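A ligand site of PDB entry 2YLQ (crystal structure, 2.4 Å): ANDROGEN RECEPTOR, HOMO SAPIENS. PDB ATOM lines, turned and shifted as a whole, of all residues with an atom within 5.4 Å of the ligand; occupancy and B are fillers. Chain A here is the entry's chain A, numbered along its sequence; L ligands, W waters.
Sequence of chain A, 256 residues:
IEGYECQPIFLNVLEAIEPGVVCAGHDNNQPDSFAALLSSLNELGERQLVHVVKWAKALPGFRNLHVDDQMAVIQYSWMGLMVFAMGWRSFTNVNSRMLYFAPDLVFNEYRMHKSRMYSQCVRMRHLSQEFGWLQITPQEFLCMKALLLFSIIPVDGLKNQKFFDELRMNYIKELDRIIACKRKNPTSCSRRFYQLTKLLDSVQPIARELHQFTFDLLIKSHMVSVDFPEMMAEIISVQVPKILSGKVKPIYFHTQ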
ATOM      1  N   LEU A  38      -5.845 -33.546   9.660  1.00  0.00           N
ATOM      2  CA  LEU A  38      -5.380 -33.078  10.988  1.00  0.00           C
ATOM      3  C   LEU A  38      -3.860 -32.940  11.138  1.00  0.00           C
ATOM      4  O   LEU A  38      -3.395 -31.988  11.795  1.00  0.00           O
ATOM      5  CB  LEU A  38      -5.989 -33.857  12.157  1.00  0.00           C
ATOM      6  CG  LEU A  38      -7.348 -33.348  12.654  1.00  0.00           C
ATOM      7  CD1 LEU A  38      -7.252 -32.041  13.423  1.00  0.00           C
ATOM      8  CD2 LEU A  38      -8.372 -33.204  11.552  1.00  0.00           C
ATOM      9  N   LEU A  41      -3.176 -29.567   9.382  1.00  0.00           N
ATOM     10  CA  LEU A  41      -3.624 -28.474  10.247  1.00  0.00           C
ATOM     11  C   LEU A  41      -2.600 -28.266  11.369  1.00  0.00           C
ATOM     12  O   LEU A  41      -2.247 -27.129  11.681  1.00  0.00           O
ATOM     13  CB  LEU A  41      -5.004 -28.769  10.846  1.00  0.00           C
ATOM     14  CG  LEU A  41      -6.247 -28.405  10.022  1.00  0.00           C
ATOM     15  CD1 LEU A  41      -7.468 -28.787  10.778  1.00  0.00           C
ATOM     16  CD2 LEU A  41      -6.349 -26.941   9.657  1.00  0.00           C
ATOM     17  N   ASN A  42      -2.118 -29.369  11.941  1.00  0.00           N
ATOM     18  CA  ASN A  42      -1.014 -29.369  12.926  1.00  0.00           C
ATOM     19  C   ASN A  42       0.311 -28.771  12.415  1.00  0.00           C
ATOM     20  O   ASN A  42       0.932 -27.958  13.111  1.00  0.00           O
ATOM     21  CB  ASN A  42      -0.781 -30.751  13.525  1.00  0.00           C
ATOM     22  CG  ASN A  42      -1.889 -31.181  14.469  1.00  0.00           C
ATOM     23  OD1 ASN A  42      -2.756 -30.381  14.840  1.00  0.00           O
ATOM     24  ND2 ASN A  42      -1.887 -32.459  14.854  1.00  0.00           N
ATOM     25  N   LEU A  44       0.508 -26.772   9.912  1.00  0.00           N
ATOM     26  CA  LEU A  44       0.134 -25.371   9.719  1.00  0.00           C
ATOM     27  C   LEU A  44       0.270 -24.606  11.039  1.00  0.00           C
ATOM     28  O   LEU A  44       0.801 -23.479  11.065  1.00  0.00           O
ATOM     29  CB  LEU A  44      -1.290 -25.248   9.224  1.00  0.00           C
ATOM     30  CG  LEU A  44      -1.679 -23.793   8.925  1.00  0.00           C
ATOM     31  CD1 LEU A  44      -0.741 -23.170   7.821  1.00  0.00           C
ATOM     32  CD2 LEU A  44      -3.170 -23.665   8.558  1.00  0.00           C
ATOM     33  N   GLY A  45      -0.221 -25.186  12.126  1.00  0.00           N
ATOM     34  CA  GLY A  45      -0.146 -24.557  13.411  1.00  0.00           C
ATOM     35  C   GLY A  45       1.291 -24.277  13.744  1.00  0.00           C
ATOM     36  O   GLY A  45       1.607 -23.167  14.128  1.00  0.00           O
ATOM     37  N   GLN A  48       2.606 -21.445  11.518  1.00  0.00           N
ATOM     38  CA  GLN A  48       2.080 -20.181  11.969  1.00  0.00           C
ATOM     39  C   GLN A  48       2.697 -19.711  13.294  1.00  0.00           C
ATOM     40  O   GLN A  48       2.900 -18.539  13.455  1.00  0.00           O
ATOM     41  CB  GLN A  48       0.575 -20.197  11.999  1.00  0.00           C
ATOM     42  CG  GLN A  48      -0.017 -20.221  10.645  1.00  0.00           C
ATOM     43  CD  GLN A  48      -1.479 -19.845  10.688  1.00  0.00           C
ATOM     44  OE1 GLN A  48      -1.996 -19.332  11.690  1.00  0.00           O
ATOM     45  NE2 GLN A  48      -2.174 -20.096   9.594  1.00  0.00           N
ATOM     46  N   TRP A  78      -2.292 -18.141  21.212  1.00  0.00           N
ATOM     47  CA  TRP A  78      -2.147 -18.489  19.798  1.00  0.00           C
ATOM     48  C   TRP A  78      -3.412 -18.994  19.094  1.00  0.00           C
ATOM     49  O   TRP A  78      -3.749 -18.518  17.998  1.00  0.00           O
ATOM     50  CB  TRP A  78      -0.986 -19.437  19.553  1.00  0.00           C
ATOM     51  CG  TRP A  78      -1.103 -20.666  20.340  1.00  0.00           C
ATOM     52  CD1 TRP A  78      -0.683 -20.865  21.611  1.00  0.00           C
ATOM     53  CD2 TRP A  78      -1.666 -21.913  19.898  1.00  0.00           C
ATOM     54  NE1 TRP A  78      -0.951 -22.167  22.014  1.00  0.00           N
ATOM     55  CE2 TRP A  78      -1.566 -22.822  20.978  1.00  0.00           C
ATOM     56  CE3 TRP A  78      -2.248 -22.340  18.708  1.00  0.00           C
ATOM     57  CZ2 TRP A  78      -2.031 -24.150  20.907  1.00  0.00           C
ATOM     58  CZ3 TRP A  78      -2.711 -23.667  18.622  1.00  0.00           C
ATOM     59  CH2 TRP A  78      -2.596 -24.555  19.720  1.00  0.00           C
ATOM     60  N   MET A  79      -4.124 -19.896  19.738  1.00  0.00           N
ATOM     61  CA  MET A  79      -5.362 -20.450  19.184  1.00  0.00           C
ATOM     62  C   MET A  79      -6.332 -19.364  18.768  1.00  0.00           C
ATOM     63  O   MET A  79      -6.806 -19.374  17.635  1.00  0.00           O
ATOM     64  CB  MET A  79      -6.056 -21.463  20.137  1.00  0.00           C
ATOM     65  CG  MET A  79      -7.239 -22.169  19.496  1.00  0.00           C
ATOM     66  SD  MET A  79      -6.710 -23.405  18.283  1.00  0.00           S
ATOM     67  CE  MET A  79      -6.066 -24.692  19.371  1.00  0.00           C
ATOM     68  N   MET A  82      -4.703 -17.073  15.607  1.00  0.00           N
ATOM     69  CA  MET A  82      -4.855 -17.879  14.410  1.00  0.00           C
ATOM     70  C   MET A  82      -6.281 -18.127  13.923  1.00  0.00           C
ATOM     71  O   MET A  82      -6.573 -17.948  12.751  1.00  0.00           O
ATOM     72  CB  MET A  82      -4.100 -19.174  14.611  1.00  0.00           C
ATOM     73  CG  MET A  82      -2.596 -18.935  14.815  1.00  0.00           C
ATOM     74  SD  MET A  82      -1.844 -20.503  15.150  1.00  0.00           S
ATOM     75  CE  MET A  82      -0.126 -20.149  15.492  1.00  0.00           C
ATOM     76  N   VAL A  83      -7.197 -18.456  14.831  1.00  0.00           N
ATOM     77  CA  VAL A  83      -8.593 -18.652  14.450  1.00  0.00           C
ATOM     78  C   VAL A  83      -9.142 -17.370  13.888  1.00  0.00           C
ATOM     79  O   VAL A  83      -9.819 -17.341  12.855  1.00  0.00           O
ATOM     80  CB  VAL A  83      -9.442 -19.097  15.638  1.00  0.00           C
ATOM     81  CG1 VAL A  83     -10.919 -18.923  15.376  1.00  0.00           C
ATOM     82  CG2 VAL A  83      -9.143 -20.538  15.942  1.00  0.00           C
ATOM     83  N   MET A  86      -7.641 -16.458  10.506  1.00  0.00           N
ATOM     84  CA  MET A  86      -8.148 -17.432   9.537  1.00  0.00           C
ATOM     85  C   MET A  86      -9.564 -17.014   9.045  1.00  0.00           C
ATOM     86  O   MET A  86      -9.862 -17.112   7.857  1.00  0.00           O
ATOM     87  CB  MET A  86      -8.127 -18.848  10.109  1.00  0.00           C
ATOM     88  CG  MET A  86      -8.530 -19.933   9.131  1.00  0.00           C
ATOM     89  SD  MET A  86     -10.316 -20.069   9.043  1.00  0.00           S
ATOM     90  CE  MET A  86     -10.618 -21.058  10.528  1.00  0.00           C
ATOM     91  N   ARG A  89      -9.066 -14.047   6.696  1.00  0.00           N
ATOM     92  CA  ARG A  89      -8.635 -14.618   5.423  1.00  0.00           C
ATOM     93  C   ARG A  89      -9.818 -15.216   4.696  1.00  0.00           C
ATOM     94  O   ARG A  89      -9.949 -15.061   3.484  1.00  0.00           O
ATOM     95  CB  ARG A  89      -7.646 -15.767   5.617  1.00  0.00           C
ATOM     96  CG  ARG A  89      -6.264 -15.343   5.967  1.00  0.00           C
ATOM     97  CD  ARG A  89      -5.301 -16.475   5.688  1.00  0.00           C
ATOM     98  NE  ARG A  89      -5.508 -17.653   6.518  1.00  0.00           N
ATOM     99  CZ  ARG A  89      -5.028 -17.806   7.770  1.00  0.00           C
ATOM    100  NH1 ARG A  89      -4.323 -16.838   8.377  1.00  0.00           N
ATOM    101  NH2 ARG A  89      -5.254 -18.943   8.415  1.00  0.00           N
ATOM    102  N   PHE A 101      -7.916 -21.962   5.703  1.00  0.00           N
ATOM    103  CA  PHE A 101      -6.790 -22.142   6.594  1.00  0.00           C
ATOM    104  C   PHE A 101      -5.531 -21.663   5.948  1.00  0.00           C
ATOM    105  O   PHE A 101      -4.774 -20.958   6.582  1.00  0.00           O
ATOM    106  CB  PHE A 101      -6.664 -23.599   7.034  1.00  0.00           C
ATOM    107  CG  PHE A 101      -7.760 -24.003   7.917  1.00  0.00           C
ATOM    108  CD1 PHE A 101      -7.714 -23.673   9.274  1.00  0.00           C
ATOM    109  CD2 PHE A 101      -8.867 -24.662   7.415  1.00  0.00           C
ATOM    110  CE1 PHE A 101      -8.771 -24.030  10.122  1.00  0.00           C
ATOM    111  CE2 PHE A 101      -9.925 -25.036   8.262  1.00  0.00           C
ATOM    112  CZ  PHE A 101      -9.873 -24.712   9.634  1.00  0.00           C
ATOM    113  N   MET A 117     -14.675 -32.278  12.856  1.00  0.00           N
ATOM    114  CA  MET A 117     -14.765 -31.023  13.586  1.00  0.00           C
ATOM    115  C   MET A 117     -15.883 -30.194  13.074  1.00  0.00           C
ATOM    116  O   MET A 117     -15.831 -28.945  13.171  1.00  0.00           O
ATOM    117  CB  MET A 117     -13.540 -30.166  13.328  1.00  0.00           C
ATOM    118  CG  MET A 117     -12.225 -30.685  13.816  1.00  0.00           C
ATOM    119  SD  MET A 117     -11.207 -29.199  13.940  1.00  0.00           S
ATOM    120  CE  MET A 117     -10.533 -29.014  12.311  1.00  0.00           C
ATOM    121  N   MET A 124     -16.486 -21.479  13.434  1.00  0.00           N
ATOM    122  CA  MET A 124     -15.502 -20.617  12.777  1.00  0.00           C
ATOM    123  C   MET A 124     -16.107 -19.908  11.562  1.00  0.00           C
ATOM    124  O   MET A 124     -15.862 -18.699  11.373  1.00  0.00           O
ATOM    125  CB  MET A 124     -14.253 -21.392  12.416  1.00  0.00           C
ATOM    126  CG  MET A 124     -13.576 -21.987  13.639  1.00  0.00           C
ATOM    127  SD  MET A 124     -11.991 -22.763  13.288  1.00  0.00           S
ATOM    128  CE  MET A 124     -12.424 -24.478  13.092  1.00  0.00           C
ATOM    129  N   LEU A 210     -11.618 -25.584  20.525  1.00  0.00           N
ATOM    130  CA  LEU A 210     -10.471 -26.115  19.788  1.00  0.00           C
ATOM    131  C   LEU A 210      -9.363 -26.563  20.727  1.00  0.00           C
ATOM    132  O   LEU A 210      -8.609 -27.510  20.413  1.00  0.00           O
ATOM    133  CB  LEU A 210      -9.974 -25.108  18.719  1.00  0.00           C
ATOM    134  CG  LEU A 210     -11.124 -24.699  17.774  1.00  0.00           C
ATOM    135  CD1 LEU A 210     -10.932 -23.309  17.089  1.00  0.00           C
ATOM    136  CD2 LEU A 210     -11.467 -25.780  16.703  1.00  0.00           C
ATOM    137  N   PHE A 213     -10.580 -30.089  21.906  1.00  0.00           N
ATOM    138  CA  PHE A 213     -10.441 -30.998  20.795  1.00  0.00           C
ATOM    139  C   PHE A 213      -8.980 -31.366  20.517  1.00  0.00           C
ATOM    140  O   PHE A 213      -8.640 -32.556  20.455  1.00  0.00           O
ATOM    141  CB  PHE A 213     -11.105 -30.370  19.583  1.00  0.00           C
ATOM    142  CG  PHE A 213     -11.167 -31.288  18.398  1.00  0.00           C
ATOM    143  CD1 PHE A 213     -10.017 -31.534  17.635  1.00  0.00           C
ATOM    144  CD2 PHE A 213     -12.367 -31.920  18.058  1.00  0.00           C
ATOM    145  CE1 PHE A 213     -10.060 -32.401  16.547  1.00  0.00           C
ATOM    146  CE2 PHE A 213     -12.426 -32.792  16.969  1.00  0.00           C
ATOM    147  CZ  PHE A 213     -11.258 -33.032  16.194  1.00  0.00           C
ATOM    148  N   THR A 214      -8.104 -30.377  20.397  1.00  0.00           N
ATOM    149  CA  THR A 214      -6.720 -30.684  20.085  1.00  0.00           C
ATOM    150  C   THR A 214      -6.104 -31.469  21.219  1.00  0.00           C
ATOM    151  O   THR A 214      -5.242 -32.295  20.995  1.00  0.00           O
ATOM    152  CB  THR A 214      -5.865 -29.400  19.687  1.00  0.00           C
ATOM    153  OG1 THR A 214      -4.679 -29.808  19.004  1.00  0.00           O
ATOM    154  CG2 THR A 214      -5.429 -28.532  20.899  1.00  0.00           C
ATOM    155  N   LEU A 217      -7.240 -34.922  21.035  1.00  0.00           N
ATOM    156  CA  LEU A 217      -6.596 -35.515  19.865  1.00  0.00           C
ATOM    157  C   LEU A 217      -5.166 -35.947  20.194  1.00  0.00           C
ATOM    158  O   LEU A 217      -4.723 -37.001  19.766  1.00  0.00           O
ATOM    159  CB  LEU A 217      -6.637 -34.571  18.673  1.00  0.00           C
ATOM    160  CG  LEU A 217      -6.057 -35.148  17.353  1.00  0.00           C
ATOM    161  CD1 LEU A 217      -6.778 -36.443  17.011  1.00  0.00           C
ATOM    162  CD2 LEU A 217      -6.253 -34.183  16.251  1.00  0.00           C
ATOM    163  N   PHE A 228       1.837 -34.728  15.483  1.00  0.00           N
ATOM    164  CA  PHE A 228       1.969 -33.420  16.121  1.00  0.00           C
ATOM    165  C   PHE A 228       3.427 -33.066  16.076  1.00  0.00           C
ATOM    166  O   PHE A 228       4.266 -33.840  16.530  1.00  0.00           O
ATOM    167  CB  PHE A 228       1.460 -33.470  17.563  1.00  0.00           C
ATOM    168  CG  PHE A 228      -0.040 -33.353  17.694  1.00  0.00           C
ATOM    169  CD1 PHE A 228      -0.868 -34.462  17.478  1.00  0.00           C
ATOM    170  CD2 PHE A 228      -0.635 -32.145  18.020  1.00  0.00           C
ATOM    171  CE1 PHE A 228      -2.274 -34.353  17.612  1.00  0.00           C
ATOM    172  CE2 PHE A 228      -2.050 -32.030  18.153  1.00  0.00           C
ATOM    173  CZ  PHE A 228      -2.865 -33.135  17.968  1.00  0.00           C
ATOM    174  N   MET A 232       4.028 -27.948  18.850  1.00  0.00           N
ATOM    175  CA  MET A 232       2.571 -28.098  19.077  1.00  0.00           C
ATOM    176  C   MET A 232       2.336 -29.136  20.183  1.00  0.00           C
ATOM    177  O   MET A 232       1.459 -28.966  21.059  1.00  0.00           O
ATOM    178  CB  MET A 232       1.832 -28.511  17.791  1.00  0.00           C
ATOM    179  CG  MET A 232       1.785 -27.446  16.712  1.00  0.00           C
ATOM    180  SD  MET A 232       0.665 -26.096  17.091  1.00  0.00           S
ATOM    181  CE  MET A 232      -0.939 -26.824  16.671  1.00  0.00           C
ATOM    182  N   ILE A 236       0.615 -28.141  23.695  1.00  0.00           N
ATOM    183  CA  ILE A 236      -0.697 -28.734  23.915  1.00  0.00           C
ATOM    184  C   ILE A 236      -0.673 -29.560  25.176  1.00  0.00           C
ATOM    185  O   ILE A 236      -1.670 -29.619  25.862  1.00  0.00           O
ATOM    186  CB  ILE A 236      -1.225 -29.412  22.653  1.00  0.00           C
ATOM    187  CG1 ILE A 236      -1.616 -28.281  21.651  1.00  0.00           C
ATOM    188  CG2 ILE A 236      -2.400 -30.330  22.956  1.00  0.00           C
ATOM    189  CD1 ILE A 236      -1.748 -28.702  20.200  1.00  0.00           C
HETATM  190  C1  LIG L   1      -3.983 -23.629  12.401  1.00  0.00           C
HETATM  191  C2  LIG L   1      -3.835 -22.197  11.899  1.00  0.00           C
HETATM  192  C3  LIG L   1      -5.214 -21.704  11.495  1.00  0.00           C
HETATM  193  O1  LIG L   1      -5.352 -20.950  10.523  1.00  0.00           O
HETATM  194  C4  LIG L   1      -6.382 -22.148  12.282  1.00  0.00           C
HETATM  195  C5  LIG L   1      -6.271 -23.053  13.278  1.00  0.00           C
HETATM  196  C6  LIG L   1      -7.512 -23.408  14.075  1.00  0.00           C
HETATM  197  C7  LIG L   1      -7.643 -24.913  14.133  1.00  0.00           C
HETATM  198  C8  LIG L   1      -6.439 -25.531  14.774  1.00  0.00           C
HETATM  199  C9  LIG L   1      -5.211 -25.217  13.894  1.00  0.00           C
HETATM  200  C10 LIG L   1      -4.963 -23.730  13.607  1.00  0.00           C
HETATM  201  C11 LIG L   1      -3.913 -25.909  14.378  1.00  0.00           C
HETATM  202  C12 LIG L   1      -4.106 -27.429  14.612  1.00  0.00           C
HETATM  203  C13 LIG L   1      -5.323 -27.730  15.466  1.00  0.00           C
HETATM  204  C14 LIG L   1      -6.553 -27.061  14.853  1.00  0.00           C
HETATM  205  C15 LIG L   1      -7.770 -27.733  15.507  1.00  0.00           C
HETATM  206  C16 LIG L   1      -7.269 -29.131  15.887  1.00  0.00           C
HETATM  207  C17 LIG L   1      -5.810 -29.182  15.449  1.00  0.00           C
HETATM  208  O2  LIG L   1      -5.070 -30.102  16.261  1.00  0.00           O
HETATM  209  C18 LIG L   1      -5.068 -27.182  16.881  1.00  0.00           C
HETATM  210  C19 LIG L   1      -4.356 -23.016  14.823  1.00  0.00           C
HETATM  211  O   HOH W   1      -4.213 -18.060  11.224  1.00  0.00           O
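Residues that only touch the ligand: Leu 41, Met 86, Met 82, Phe 101, Met 79, Leu 44, Leu 38, Val 83 and Met 232.
Hydrophobic or aromatic side chains within 4 Å of the ligand: Leu 38, Leu 44, Met 79, Met 82, Val 83, Met 86, Phe 101 and Met 232.
An oxygen (O1) of the ligand sits at hydrogen-bond distance from the side-chain amide nitrogen (NE2) of Gln 48.
An oxygen (O1) of the ligand lies within hydrogen-bond range of the guanidinium group of Arg 89 (2.9 Å).
The side-chain amide oxygen of Asn 42 is in hydrogen-bond range of an oxygen (O2) of the ligand (2.7 Å).
O2 of the ligand is in hydrogen-bond range of OG1 of Thr 214, at 2.8 Å.
OE1 of Gln 48 lies close to SD of Met 82 (3.7 Å).
The side-chain amide nitrogen (NE2) of Gln 48 sits close to the guanidinium group (NH2) of Arg 89, at 3.5 Å.
The guanidinium group of Arg 89 lies within hydrogen-bond range of the backbone carbonyl oxygen of Phe 101, 2.8 Å away.
ND2 of Asn 42 lies close to O of Leu 38, at 3.4 Å.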
